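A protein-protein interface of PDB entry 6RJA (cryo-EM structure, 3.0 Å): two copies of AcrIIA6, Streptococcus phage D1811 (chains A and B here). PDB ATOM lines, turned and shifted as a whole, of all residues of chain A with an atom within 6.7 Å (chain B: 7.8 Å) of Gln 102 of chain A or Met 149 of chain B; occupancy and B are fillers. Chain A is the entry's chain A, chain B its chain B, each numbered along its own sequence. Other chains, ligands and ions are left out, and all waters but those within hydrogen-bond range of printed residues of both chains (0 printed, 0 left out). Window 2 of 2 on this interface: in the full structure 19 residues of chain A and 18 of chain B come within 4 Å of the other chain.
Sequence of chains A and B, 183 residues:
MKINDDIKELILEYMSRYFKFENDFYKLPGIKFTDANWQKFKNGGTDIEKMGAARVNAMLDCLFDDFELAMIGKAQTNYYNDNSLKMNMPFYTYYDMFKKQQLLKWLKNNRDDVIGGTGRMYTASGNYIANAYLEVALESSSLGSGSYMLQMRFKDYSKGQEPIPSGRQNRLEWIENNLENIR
The backbone carbonyl oxygen (O) of Tyr 148 of chain B lies within hydrogen-bond range of the side-chain amino group (NZ) of Lys 74 of chain A.
N of Met 149 of chain B sits at hydrogen-bond distance from O of Ser 141 of chain B (2.8 Å).
Ala 70 of chain A touches Asp 66 of chain B (CB to O, 3.3 Å). Met 71 of chain A touches Met 149 of chain B. CE of Lys 74 of chain A touches OD2 of Asp 66 of chain B (3.7 Å). Lys 74 of chain A touches Leu 143 of chain B (CD to CD1, 3.9 Å). CD1 of Leu 143 of chain B touches CZ of Phe 98 of chain A, 3.9 Å away. Gln 102 of chain A touches Met 149 of chain B (NE2 to CG, 3.96 Å).
Gln 102 of chain A touches just one residue of chain B: Met 149. Of the printed residues of chain A, Met 149 of chain B touches Met 71 and Gln 102. Of the printed residues of chain B, Lys 74 of chain A touches Asp 66, Leu 143 and Tyr 148. Printed residues of chain B within 4 Å of Met 71 of chain A: Met 149. Asp 65 of chain B touches none of the printed residues of chain A. Trp 106 of chain B touches none of the printed residues of chain A. The nearest residue of chain B that does not touch Gln 102 of chain A is Leu 143 of chain B (4.1 Å). The nearest printed residue of chain B that does not touch Ala 70 of chain A is Met 149 of chain B (4.1 Å).
Printed residues of chain A that touch a printed residue of chain B: Ala 70, Met 71, Lys 74, Phe 98 and Gln 102. Hydrophobic or aromatic side chains of chain A within 4 Å of the printed part of chain B: Ala 70, Met 71 and Phe 98. Hydrophobic or aromatic side chains of chain B within 4 Å of the printed part of chain A: Leu 143 and Met 149. Among the printed residues, 7 pairs touch across the chains. Among the printed residues, no Asp or Glu carboxylate lies within 4 Å of a Lys or Arg side-chain nitrogen of the other chain.
Positions printed for both chains: 67, 106 and 152. Of the 7 pairs that touch across the chains among the printed residues, none has its exchanged pair printed and touching as well.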
ATOM      1  N   PHE A  67      -1.373 -12.474  -0.621  1.00  0.00           N
ATOM      2  CA  PHE A  67      -1.657 -13.155   0.637  1.00  0.00           C
ATOM      3  C   PHE A  67      -0.415 -13.228   1.519  1.00  0.00           C
ATOM      4  O   PHE A  67      -0.515 -13.258   2.756  1.00  0.00           O
ATOM      5  CB  PHE A  67      -2.197 -14.547   0.324  1.00  0.00           C
ATOM      6  CG  PHE A  67      -2.752 -15.275   1.505  1.00  0.00           C
ATOM      7  CD1 PHE A  67      -3.817 -14.759   2.212  1.00  0.00           C
ATOM      8  CD2 PHE A  67      -2.233 -16.494   1.881  1.00  0.00           C
ATOM      9  CE1 PHE A  67      -4.333 -15.432   3.288  1.00  0.00           C
ATOM     10  CE2 PHE A  67      -2.751 -17.169   2.954  1.00  0.00           C
ATOM     11  CZ  PHE A  67      -3.800 -16.635   3.657  1.00  0.00           C
ATOM     12  N   ALA A  70       0.035 -10.191   3.843  1.00  0.00           N
ATOM     13  CA  ALA A  70      -0.806 -10.383   5.020  1.00  0.00           C
ATOM     14  C   ALA A  70      -0.162 -11.339   6.015  1.00  0.00           C
ATOM     15  O   ALA A  70      -0.200 -11.105   7.232  1.00  0.00           O
ATOM     16  CB  ALA A  70      -2.175 -10.904   4.595  1.00  0.00           C
ATOM     17  N   MET A  71       0.444 -12.419   5.517  1.00  0.00           N
ATOM     18  CA  MET A  71       1.126 -13.333   6.429  1.00  0.00           C
ATOM     19  C   MET A  71       2.383 -12.713   7.035  1.00  0.00           C
ATOM     20  O   MET A  71       2.752 -13.062   8.160  1.00  0.00           O
ATOM     21  CB  MET A  71       1.465 -14.641   5.722  1.00  0.00           C
ATOM     22  CG  MET A  71       0.283 -15.558   5.550  1.00  0.00           C
ATOM     23  SD  MET A  71       0.769 -17.251   5.231  1.00  0.00           S
ATOM     24  CE  MET A  71       1.596 -17.051   3.669  1.00  0.00           C
ATOM     25  N   ILE A  72       3.036 -11.786   6.325  1.00  0.00           N
ATOM     26  CA  ILE A  72       4.154 -11.037   6.903  1.00  0.00           C
ATOM     27  C   ILE A  72       3.670 -10.180   8.064  1.00  0.00           C
ATOM     28  O   ILE A  72       4.306 -10.136   9.124  1.00  0.00           O
ATOM     29  CB  ILE A  72       4.855 -10.186   5.826  1.00  0.00           C
ATOM     30  CG1 ILE A  72       5.720 -11.052   4.924  1.00  0.00           C
ATOM     31  CG2 ILE A  72       5.758  -9.143   6.440  1.00  0.00           C
ATOM     32  CD1 ILE A  72       6.288 -10.308   3.759  1.00  0.00           C
ATOM     33  N   LYS A  74       0.999 -10.765   9.971  1.00  0.00           N
ATOM     34  CA  LYS A  74       0.609 -11.621  11.092  1.00  0.00           C
ATOM     35  C   LYS A  74       1.819 -12.228  11.798  1.00  0.00           C
ATOM     36  O   LYS A  74       1.834 -12.346  13.032  1.00  0.00           O
ATOM     37  CB  LYS A  74      -0.331 -12.715  10.606  1.00  0.00           C
ATOM     38  CG  LYS A  74      -1.656 -12.196  10.132  1.00  0.00           C
ATOM     39  CD  LYS A  74      -2.617 -12.070  11.280  1.00  0.00           C
ATOM     40  CE  LYS A  74      -3.928 -11.492  10.823  1.00  0.00           C
ATOM     41  NZ  LYS A  74      -4.832 -11.263  11.972  1.00  0.00           N
ATOM     42  N   MET A  97       8.714 -20.522   8.791  1.00  0.00           N
ATOM     43  CA  MET A  97       7.957 -21.421   9.666  1.00  0.00           C
ATOM     44  C   MET A  97       6.458 -21.133   9.625  1.00  0.00           C
ATOM     45  O   MET A  97       5.640 -22.064   9.555  1.00  0.00           O
ATOM     46  CB  MET A  97       8.473 -21.310  11.097  1.00  0.00           C
ATOM     47  CG  MET A  97       9.890 -21.796  11.286  1.00  0.00           C
ATOM     48  SD  MET A  97      10.619 -21.265  12.847  1.00  0.00           S
ATOM     49  CE  MET A  97       9.961 -22.489  13.975  1.00  0.00           C
ATOM     50  N   PHE A  98       6.088 -19.848   9.664  1.00  0.00           N
ATOM     51  CA  PHE A  98       4.688 -19.431   9.565  1.00  0.00           C
ATOM     52  C   PHE A  98       4.067 -19.863   8.238  1.00  0.00           C
ATOM     53  O   PHE A  98       2.924 -20.354   8.197  1.00  0.00           O
ATOM     54  CB  PHE A  98       4.626 -17.910   9.727  1.00  0.00           C
ATOM     55  CG  PHE A  98       3.258 -17.365  10.001  1.00  0.00           C
ATOM     56  CD1 PHE A  98       2.833 -17.159  11.294  1.00  0.00           C
ATOM     57  CD2 PHE A  98       2.416 -17.008   8.964  1.00  0.00           C
ATOM     58  CE1 PHE A  98       1.586 -16.646  11.548  1.00  0.00           C
ATOM     59  CE2 PHE A  98       1.168 -16.496   9.218  1.00  0.00           C
ATOM     60  CZ  PHE A  98       0.756 -16.315  10.506  1.00  0.00           C
ATOM     61  N   LYS A  99       4.827 -19.729   7.151  1.00  0.00           N
ATOM     62  CA  LYS A  99       4.323 -20.073   5.828  1.00  0.00           C
ATOM     63  C   LYS A  99       4.093 -21.575   5.688  1.00  0.00           C
ATOM     64  O   LYS A  99       3.070 -22.009   5.137  1.00  0.00           O
ATOM     65  CB  LYS A  99       5.312 -19.558   4.786  1.00  0.00           C
ATOM     66  CG  LYS A  99       4.788 -19.423   3.392  1.00  0.00           C
ATOM     67  CD  LYS A  99       5.759 -18.624   2.559  1.00  0.00           C
ATOM     68  CE  LYS A  99       7.063 -19.363   2.394  1.00  0.00           C
ATOM     69  NZ  LYS A  99       7.986 -18.658   1.470  1.00  0.00           N
ATOM     70  N   LYS A 100       5.005 -22.391   6.223  1.00  0.00           N
ATOM     71  CA  LYS A 100       4.796 -23.832   6.117  1.00  0.00           C
ATOM     72  C   LYS A 100       3.706 -24.327   7.063  1.00  0.00           C
ATOM     73  O   LYS A 100       3.041 -25.326   6.760  1.00  0.00           O
ATOM     74  CB  LYS A 100       6.106 -24.579   6.342  1.00  0.00           C
ATOM     75  CG  LYS A 100       6.060 -26.009   5.840  1.00  0.00           C
ATOM     76  CD  LYS A 100       7.423 -26.639   5.792  1.00  0.00           C
ATOM     77  CE  LYS A 100       8.237 -25.968   4.711  1.00  0.00           C
ATOM     78  NZ  LYS A 100       7.527 -26.018   3.405  1.00  0.00           N
ATOM     79  N   GLN A 101       3.479 -23.635   8.187  1.00  0.00           N
ATOM     80  CA  GLN A 101       2.327 -23.961   9.029  1.00  0.00           C
ATOM     81  C   GLN A 101       1.014 -23.731   8.290  1.00  0.00           C
ATOM     82  O   GLN A 101       0.092 -24.557   8.371  1.00  0.00           O
ATOM     83  CB  GLN A 101       2.358 -23.138  10.313  1.00  0.00           C
ATOM     84  CG  GLN A 101       3.285 -23.683  11.382  1.00  0.00           C
ATOM     85  CD  GLN A 101       3.333 -22.803  12.616  1.00  0.00           C
ATOM     86  OE1 GLN A 101       4.340 -22.754  13.322  1.00  0.00           O
ATOM     87  NE2 GLN A 101       2.241 -22.100  12.881  1.00  0.00           N
ATOM     88  N   GLN A 102       0.925 -22.630   7.537  1.00  0.00           N
ATOM     89  CA  GLN A 102      -0.283 -22.381   6.749  1.00  0.00           C
ATOM     90  C   GLN A 102      -0.461 -23.407   5.632  1.00  0.00           C
ATOM     91  O   GLN A 102      -1.591 -23.829   5.346  1.00  0.00           O
ATOM     92  CB  GLN A 102      -0.256 -20.973   6.169  1.00  0.00           C
ATOM     93  CG  GLN A 102      -1.623 -20.445   5.824  1.00  0.00           C
ATOM     94  CD  GLN A 102      -2.367 -19.965   7.042  1.00  0.00           C
ATOM     95  OE1 GLN A 102      -1.761 -19.609   8.050  1.00  0.00           O
ATOM     96  NE2 GLN A 102      -3.688 -19.963   6.965  1.00  0.00           N
ATOM     97  N   LEU A 103       0.642 -23.839   5.010  1.00  0.00           N
ATOM     98  CA  LEU A 103       0.547 -24.866   3.968  1.00  0.00           C
ATOM     99  C   LEU A 103       0.077 -26.204   4.531  1.00  0.00           C
ATOM    100  O   LEU A 103      -0.733 -26.899   3.903  1.00  0.00           O
ATOM    101  CB  LEU A 103       1.890 -25.028   3.260  1.00  0.00           C
ATOM    102  CG  LEU A 103       1.987 -26.149   2.225  1.00  0.00           C
ATOM    103  CD1 LEU A 103       1.073 -25.874   1.049  1.00  0.00           C
ATOM    104  CD2 LEU A 103       3.410 -26.333   1.763  1.00  0.00           C
ATOM    105  N   LEU A 104       0.560 -26.574   5.719  1.00  0.00           N
ATOM    106  CA  LEU A 104       0.133 -27.829   6.332  1.00  0.00           C
ATOM    107  C   LEU A 104      -1.332 -27.785   6.745  1.00  0.00           C
ATOM    108  O   LEU A 104      -2.037 -28.798   6.649  1.00  0.00           O
ATOM    109  CB  LEU A 104       1.016 -28.148   7.530  1.00  0.00           C
ATOM    110  CG  LEU A 104       2.370 -28.727   7.151  1.00  0.00           C
ATOM    111  CD1 LEU A 104       3.357 -28.537   8.273  1.00  0.00           C
ATOM    112  CD2 LEU A 104       2.194 -30.186   6.850  1.00  0.00           C
ATOM    113  N   LYS A 105      -1.811 -26.620   7.194  1.00  0.00           N
ATOM    114  CA  LYS A 105      -3.239 -26.469   7.477  1.00  0.00           C
ATOM    115  C   LYS A 105      -4.082 -26.624   6.214  1.00  0.00           C
ATOM    116  O   LYS A 105      -5.159 -27.238   6.250  1.00  0.00           O
ATOM    117  CB  LYS A 105      -3.500 -25.116   8.133  1.00  0.00           C
ATOM    118  CG  LYS A 105      -4.938 -24.889   8.537  1.00  0.00           C
ATOM    119  CD  LYS A 105      -5.164 -23.462   8.981  1.00  0.00           C
ATOM    120  CE  LYS A 105      -4.315 -23.127  10.193  1.00  0.00           C
ATOM    121  NZ  LYS A 105      -4.646 -23.989  11.357  1.00  0.00           N
ATOM    122  N   TRP A 106      -3.596 -26.089   5.085  1.00  0.00           N
ATOM    123  CA  TRP A 106      -4.286 -26.274   3.808  1.00  0.00           C
ATOM    124  C   TRP A 106      -4.346 -27.739   3.402  1.00  0.00           C
ATOM    125  O   TRP A 106      -5.378 -28.215   2.920  1.00  0.00           O
ATOM    126  CB  TRP A 106      -3.589 -25.495   2.699  1.00  0.00           C
ATOM    127  CG  TRP A 106      -3.824 -24.042   2.688  1.00  0.00           C
ATOM    128  CD1 TRP A 106      -4.443 -23.300   3.638  1.00  0.00           C
ATOM    129  CD2 TRP A 106      -3.433 -23.135   1.661  1.00  0.00           C
ATOM    130  NE1 TRP A 106      -4.464 -21.982   3.268  1.00  0.00           N
ATOM    131  CE2 TRP A 106      -3.846 -21.857   2.054  1.00  0.00           C
ATOM    132  CE3 TRP A 106      -2.771 -23.285   0.440  1.00  0.00           C
ATOM    133  CZ2 TRP A 106      -3.620 -20.733   1.275  1.00  0.00           C
ATOM    134  CZ3 TRP A 106      -2.550 -22.173  -0.328  1.00  0.00           C
ATOM    135  CH2 TRP A 106      -2.972 -20.913   0.089  1.00  0.00           C
ATOM    136  N   LEU A 107      -3.238 -28.462   3.565  1.00  0.00           N
ATOM    137  CA  LEU A 107      -3.208 -29.861   3.149  1.00  0.00           C
ATOM    138  C   LEU A 107      -4.043 -30.743   4.063  1.00  0.00           C
ATOM    139  O   LEU A 107      -4.580 -31.761   3.616  1.00  0.00           O
ATOM    140  CB  LEU A 107      -1.774 -30.377   3.106  1.00  0.00           C
ATOM    141  CG  LEU A 107      -0.971 -29.981   1.877  1.00  0.00           C
ATOM    142  CD1 LEU A 107       0.449 -30.475   1.993  1.00  0.00           C
ATOM    143  CD2 LEU A 107      -1.635 -30.535   0.647  1.00  0.00           C
ATOM    144  N   MET A 152       0.128 -19.010  -2.375  1.00  0.00           N
ATOM    145  CA  MET A 152       1.464 -18.953  -1.808  1.00  0.00           C
ATOM    146  C   MET A 152       2.487 -19.346  -2.863  1.00  0.00           C
ATOM    147  O   MET A 152       2.147 -19.794  -3.961  1.00  0.00           O
ATOM    148  CB  MET A 152       1.580 -19.862  -0.585  1.00  0.00           C
ATOM    149  CG  MET A 152       0.848 -19.357   0.631  1.00  0.00           C
ATOM    150  SD  MET A 152       1.193 -20.358   2.081  1.00  0.00           S
ATOM    151  CE  MET A 152       0.609 -21.940   1.520  1.00  0.00           C
ATOM    152  N   ASP B  65      -7.399  -3.987   8.060  1.00  0.00           N
ATOM    153  CA  ASP B  65      -6.985  -5.289   8.560  1.00  0.00           C
ATOM    154  C   ASP B  65      -5.874  -5.849   7.667  1.00  0.00           C
ATOM    155  O   ASP B  65      -5.513  -5.272   6.641  1.00  0.00           O
ATOM    156  CB  ASP B  65      -8.190  -6.225   8.607  1.00  0.00           C
ATOM    157  CG  ASP B  65      -8.064  -7.291   9.662  1.00  0.00           C
ATOM    158  OD1 ASP B  65      -8.278  -6.975  10.848  1.00  0.00           O
ATOM    159  OD2 ASP B  65      -7.757  -8.447   9.310  1.00  0.00           O
ATOM    160  N   ASP B  66      -5.320  -6.997   8.048  1.00  0.00           N
ATOM    161  CA  ASP B  66      -4.263  -7.588   7.236  1.00  0.00           C
ATOM    162  C   ASP B  66      -4.795  -8.263   5.980  1.00  0.00           C
ATOM    163  O   ASP B  66      -4.126  -8.244   4.945  1.00  0.00           O
ATOM    164  CB  ASP B  66      -3.459  -8.581   8.068  1.00  0.00           C
ATOM    165  CG  ASP B  66      -2.403  -7.906   8.908  1.00  0.00           C
ATOM    166  OD1 ASP B  66      -1.768  -6.957   8.408  1.00  0.00           O
ATOM    167  OD2 ASP B  66      -2.218  -8.304  10.076  1.00  0.00           O
ATOM    168  N   PHE B  67      -5.985  -8.855   6.043  1.00  0.00           N
ATOM    169  CA  PHE B  67      -6.600  -9.428   4.853  1.00  0.00           C
ATOM    170  C   PHE B  67      -7.122  -8.340   3.920  1.00  0.00           C
ATOM    171  O   PHE B  67      -7.181  -8.528   2.695  1.00  0.00           O
ATOM    172  CB  PHE B  67      -7.721 -10.368   5.289  1.00  0.00           C
ATOM    173  CG  PHE B  67      -8.288 -11.205   4.191  1.00  0.00           C
ATOM    174  CD1 PHE B  67      -7.491 -12.092   3.500  1.00  0.00           C
ATOM    175  CD2 PHE B  67      -9.629 -11.135   3.879  1.00  0.00           C
ATOM    176  CE1 PHE B  67      -8.013 -12.870   2.499  1.00  0.00           C
ATOM    177  CE2 PHE B  67     -10.152 -11.914   2.883  1.00  0.00           C
ATOM    178  CZ  PHE B  67      -9.342 -12.780   2.194  1.00  0.00           C
ATOM    179  N   GLU B  68      -7.469  -7.184   4.482  1.00  0.00           N
ATOM    180  CA  GLU B  68      -8.030  -6.104   3.686  1.00  0.00           C
ATOM    181  C   GLU B  68      -6.982  -5.413   2.826  1.00  0.00           C
ATOM    182  O   GLU B  68      -7.316  -4.894   1.759  1.00  0.00           O
ATOM    183  CB  GLU B  68      -8.721  -5.108   4.601  1.00  0.00           C
ATOM    184  CG  GLU B  68     -10.101  -5.549   5.019  1.00  0.00           C
ATOM    185  CD  GLU B  68     -10.797  -4.518   5.863  1.00  0.00           C
ATOM    186  OE1 GLU B  68     -10.459  -4.414   7.055  1.00  0.00           O
ATOM    187  OE2 GLU B  68     -11.673  -3.803   5.340  1.00  0.00           O
ATOM    188  N   TRP B 106     -18.406 -15.737   1.437  1.00  0.00           N
ATOM    189  CA  TRP B 106     -18.288 -16.362   2.757  1.00  0.00           C
ATOM    190  C   TRP B 106     -19.630 -16.864   3.267  1.00  0.00           C
ATOM    191  O   TRP B 106     -19.716 -17.959   3.830  1.00  0.00           O
ATOM    192  CB  TRP B 106     -17.722 -15.378   3.772  1.00  0.00           C
ATOM    193  CG  TRP B 106     -16.273 -15.129   3.690  1.00  0.00           C
ATOM    194  CD1 TRP B 106     -15.422 -15.539   2.720  1.00  0.00           C
ATOM    195  CD2 TRP B 106     -15.493 -14.397   4.631  1.00  0.00           C
ATOM    196  NE1 TRP B 106     -14.151 -15.108   2.994  1.00  0.00           N
ATOM    197  CE2 TRP B 106     -14.171 -14.401   4.167  1.00  0.00           C
ATOM    198  CE3 TRP B 106     -15.786 -13.738   5.826  1.00  0.00           C
ATOM    199  CZ2 TRP B 106     -13.144 -13.772   4.851  1.00  0.00           C
ATOM    200  CZ3 TRP B 106     -14.768 -13.117   6.501  1.00  0.00           C
ATOM    201  CH2 TRP B 106     -13.464 -13.137   6.015  1.00  0.00           C
ATOM    202  N   ALA B 137     -15.263 -12.527  11.023  1.00  0.00           N
ATOM    203  CA  ALA B 137     -14.178 -13.466  10.779  1.00  0.00           C
ATOM    204  C   ALA B 137     -14.720 -14.855  10.480  1.00  0.00           C
ATOM    205  O   ALA B 137     -15.897 -15.149  10.690  1.00  0.00           O
ATOM    206  CB  ALA B 137     -13.223 -13.527  11.971  1.00  0.00           C
ATOM    207  N   LEU B 138     -13.836 -15.711   9.972  1.00  0.00           N
ATOM    208  CA  LEU B 138     -14.102 -17.133   9.801  1.00  0.00           C
ATOM    209  C   LEU B 138     -13.418 -17.887  10.933  1.00  0.00           C
ATOM    210  O   LEU B 138     -12.208 -17.753  11.123  1.00  0.00           O
ATOM    211  CB  LEU B 138     -13.594 -17.639   8.453  1.00  0.00           C
ATOM    212  CG  LEU B 138     -14.384 -17.307   7.194  1.00  0.00           C
ATOM    213  CD1 LEU B 138     -13.609 -17.733   5.977  1.00  0.00           C
ATOM    214  CD2 LEU B 138     -15.722 -17.990   7.225  1.00  0.00           C
ATOM    215  N   SER B 140     -12.741 -21.012  11.382  1.00  0.00           N
ATOM    216  CA  SER B 140     -11.820 -22.090  11.039  1.00  0.00           C
ATOM    217  C   SER B 140     -10.390 -21.592  10.879  1.00  0.00           C
ATOM    218  O   SER B 140      -9.443 -22.350  11.104  1.00  0.00           O
ATOM    219  CB  SER B 140     -12.278 -22.773   9.757  1.00  0.00           C
ATOM    220  OG  SER B 140     -12.200 -21.880   8.661  1.00  0.00           O
ATOM    221  N   SER B 141     -10.217 -20.334  10.490  1.00  0.00           N
ATOM    222  CA  SER B 141      -8.899 -19.769  10.213  1.00  0.00           C
ATOM    223  C   SER B 141      -8.309 -19.057  11.419  1.00  0.00           C
ATOM    224  O   SER B 141      -7.898 -17.907  11.315  1.00  0.00           O
ATOM    225  CB  SER B 141      -8.995 -18.816   9.034  1.00  0.00           C
ATOM    226  OG  SER B 141      -9.483 -17.565   9.468  1.00  0.00           O
ATOM    227  N   SER B 142      -8.245 -19.715  12.567  1.00  0.00           N
ATOM    228  CA  SER B 142      -7.699 -19.096  13.763  1.00  0.00           C
ATOM    229  C   SER B 142      -6.231 -19.461  13.905  1.00  0.00           C
ATOM    230  O   SER B 142      -5.838 -20.601  13.648  1.00  0.00           O
ATOM    231  CB  SER B 142      -8.462 -19.533  15.011  1.00  0.00           C
ATOM    232  OG  SER B 142      -8.028 -20.803  15.454  1.00  0.00           O
ATOM    233  N   LEU B 143      -5.426 -18.490  14.318  1.00  0.00           N
ATOM    234  CA  LEU B 143      -4.010 -18.736  14.548  1.00  0.00           C
ATOM    235  C   LEU B 143      -3.718 -19.060  16.004  1.00  0.00           C
ATOM    236  O   LEU B 143      -2.863 -19.903  16.295  1.00  0.00           O
ATOM    237  CB  LEU B 143      -3.185 -17.522  14.120  1.00  0.00           C
ATOM    238  CG  LEU B 143      -3.259 -17.105  12.656  1.00  0.00           C
ATOM    239  CD1 LEU B 143      -2.584 -15.772  12.469  1.00  0.00           C
ATOM    240  CD2 LEU B 143      -2.610 -18.153  11.788  1.00  0.00           C
ATOM    241  N   GLY B 144      -4.418 -18.412  16.922  1.00  0.00           N
ATOM    242  CA  GLY B 144      -4.167 -18.574  18.341  1.00  0.00           C
ATOM    243  C   GLY B 144      -4.081 -17.197  18.959  1.00  0.00           C
ATOM    244  O   GLY B 144      -3.774 -16.210  18.285  1.00  0.00           O
ATOM    245  N   GLY B 146      -6.450 -15.285  19.986  1.00  0.00           N
ATOM    246  CA  GLY B 146      -7.466 -14.367  19.510  1.00  0.00           C
ATOM    247  C   GLY B 146      -7.197 -13.734  18.168  1.00  0.00           C
ATOM    248  O   GLY B 146      -7.740 -12.664  17.888  1.00  0.00           O
ATOM    249  N   SER B 147      -6.379 -14.356  17.327  1.00  0.00           N
ATOM    250  CA  SER B 147      -6.082 -13.840  16.002  1.00  0.00           C
ATOM    251  C   SER B 147      -6.732 -14.725  14.953  1.00  0.00           C
ATOM    252  O   SER B 147      -6.805 -15.945  15.116  1.00  0.00           O
ATOM    253  CB  SER B 147      -4.576 -13.765  15.753  1.00  0.00           C
ATOM    254  OG  SER B 147      -3.981 -12.736  16.518  1.00  0.00           O
ATOM    255  N   TYR B 148      -7.207 -14.104  13.882  1.00  0.00           N
ATOM    256  CA  TYR B 148      -7.805 -14.817  12.767  1.00  0.00           C
ATOM    257  C   TYR B 148      -7.093 -14.413  11.491  1.00  0.00           C
ATOM    258  O   TYR B 148      -6.723 -13.251  11.321  1.00  0.00           O
ATOM    259  CB  TYR B 148      -9.298 -14.531  12.677  1.00  0.00           C
ATOM    260  CG  TYR B 148     -10.042 -15.095  13.854  1.00  0.00           C
ATOM    261  CD1 TYR B 148     -10.397 -16.431  13.891  1.00  0.00           C
ATOM    262  CD2 TYR B 148     -10.351 -14.304  14.948  1.00  0.00           C
ATOM    263  CE1 TYR B 148     -11.055 -16.961  14.971  1.00  0.00           C
ATOM    264  CE2 TYR B 148     -11.012 -14.827  16.035  1.00  0.00           C
ATOM    265  CZ  TYR B 148     -11.359 -16.155  16.038  1.00  0.00           C
ATOM    266  OH  TYR B 148     -12.019 -16.688  17.114  1.00  0.00           O
ATOM    267  N   MET B 149      -6.892 -15.378  10.600  1.00  0.00           N
ATOM    268  CA  MET B 149      -6.188 -15.087   9.361  1.00  0.00           C
ATOM    269  C   MET B 149      -7.081 -14.357   8.366  1.00  0.00           C
ATOM    270  O   MET B 149      -6.648 -13.388   7.739  1.00  0.00           O
ATOM    271  CB  MET B 149      -5.649 -16.383   8.761  1.00  0.00           C
ATOM    272  CG  MET B 149      -4.723 -16.191   7.582  1.00  0.00           C
ATOM    273  SD  MET B 149      -3.086 -15.602   8.028  1.00  0.00           S
ATOM    274  CE  MET B 149      -2.934 -14.222   6.911  1.00  0.00           C
ATOM    275  N   LEU B 150      -8.330 -14.788   8.220  1.00  0.00           N
ATOM    276  CA  LEU B 150      -9.284 -14.163   7.309  1.00  0.00           C
ATOM    277  C   LEU B 150     -10.294 -13.384   8.136  1.00  0.00           C
ATOM    278  O   LEU B 150     -11.117 -13.977   8.836  1.00  0.00           O
ATOM    279  CB  LEU B 150      -9.982 -15.202   6.437  1.00  0.00           C
ATOM    280  CG  LEU B 150      -9.136 -16.248   5.714  1.00  0.00           C
ATOM    281  CD1 LEU B 150     -10.013 -17.038   4.786  1.00  0.00           C
ATOM    282  CD2 LEU B 150      -8.005 -15.609   4.946  1.00  0.00           C
ATOM    283  N   GLN B 151     -10.240 -12.060   8.044  1.00  0.00           N
ATOM    284  CA  GLN B 151     -11.047 -11.191   8.886  1.00  0.00           C
ATOM    285  C   GLN B 151     -11.309  -9.888   8.156  1.00  0.00           C
ATOM    286  O   GLN B 151     -10.389  -9.309   7.579  1.00  0.00           O
ATOM    287  CB  GLN B 151     -10.339 -10.922  10.208  1.00  0.00           C
ATOM    288  CG  GLN B 151     -11.215 -10.335  11.271  1.00  0.00           C
ATOM    289  CD  GLN B 151     -10.481 -10.157  12.574  1.00  0.00           C
ATOM    290  OE1 GLN B 151      -9.267 -10.330  12.642  1.00  0.00           O
ATOM    291  NE2 GLN B 151     -11.210  -9.806  13.618  1.00  0.00           N
ATOM    292  N   MET B 152     -12.551  -9.429   8.188  1.00  0.00           N
ATOM    293  CA  MET B 152     -12.964  -8.189   7.555  1.00  0.00           C
ATOM    294  C   MET B 152     -13.613  -7.278   8.587  1.00  0.00           C
ATOM    295  O   MET B 152     -13.868  -7.669   9.729  1.00  0.00           O
ATOM    296  CB  MET B 152     -13.923  -8.455   6.397  1.00  0.00           C
ATOM    297  CG  MET B 152     -13.271  -9.067   5.183  1.00  0.00           C
ATOM    298  SD  MET B 152     -14.405  -9.162   3.794  1.00  0.00           S
ATOM    299  CE  MET B 152     -15.676 -10.186   4.494  1.00  0.00           C
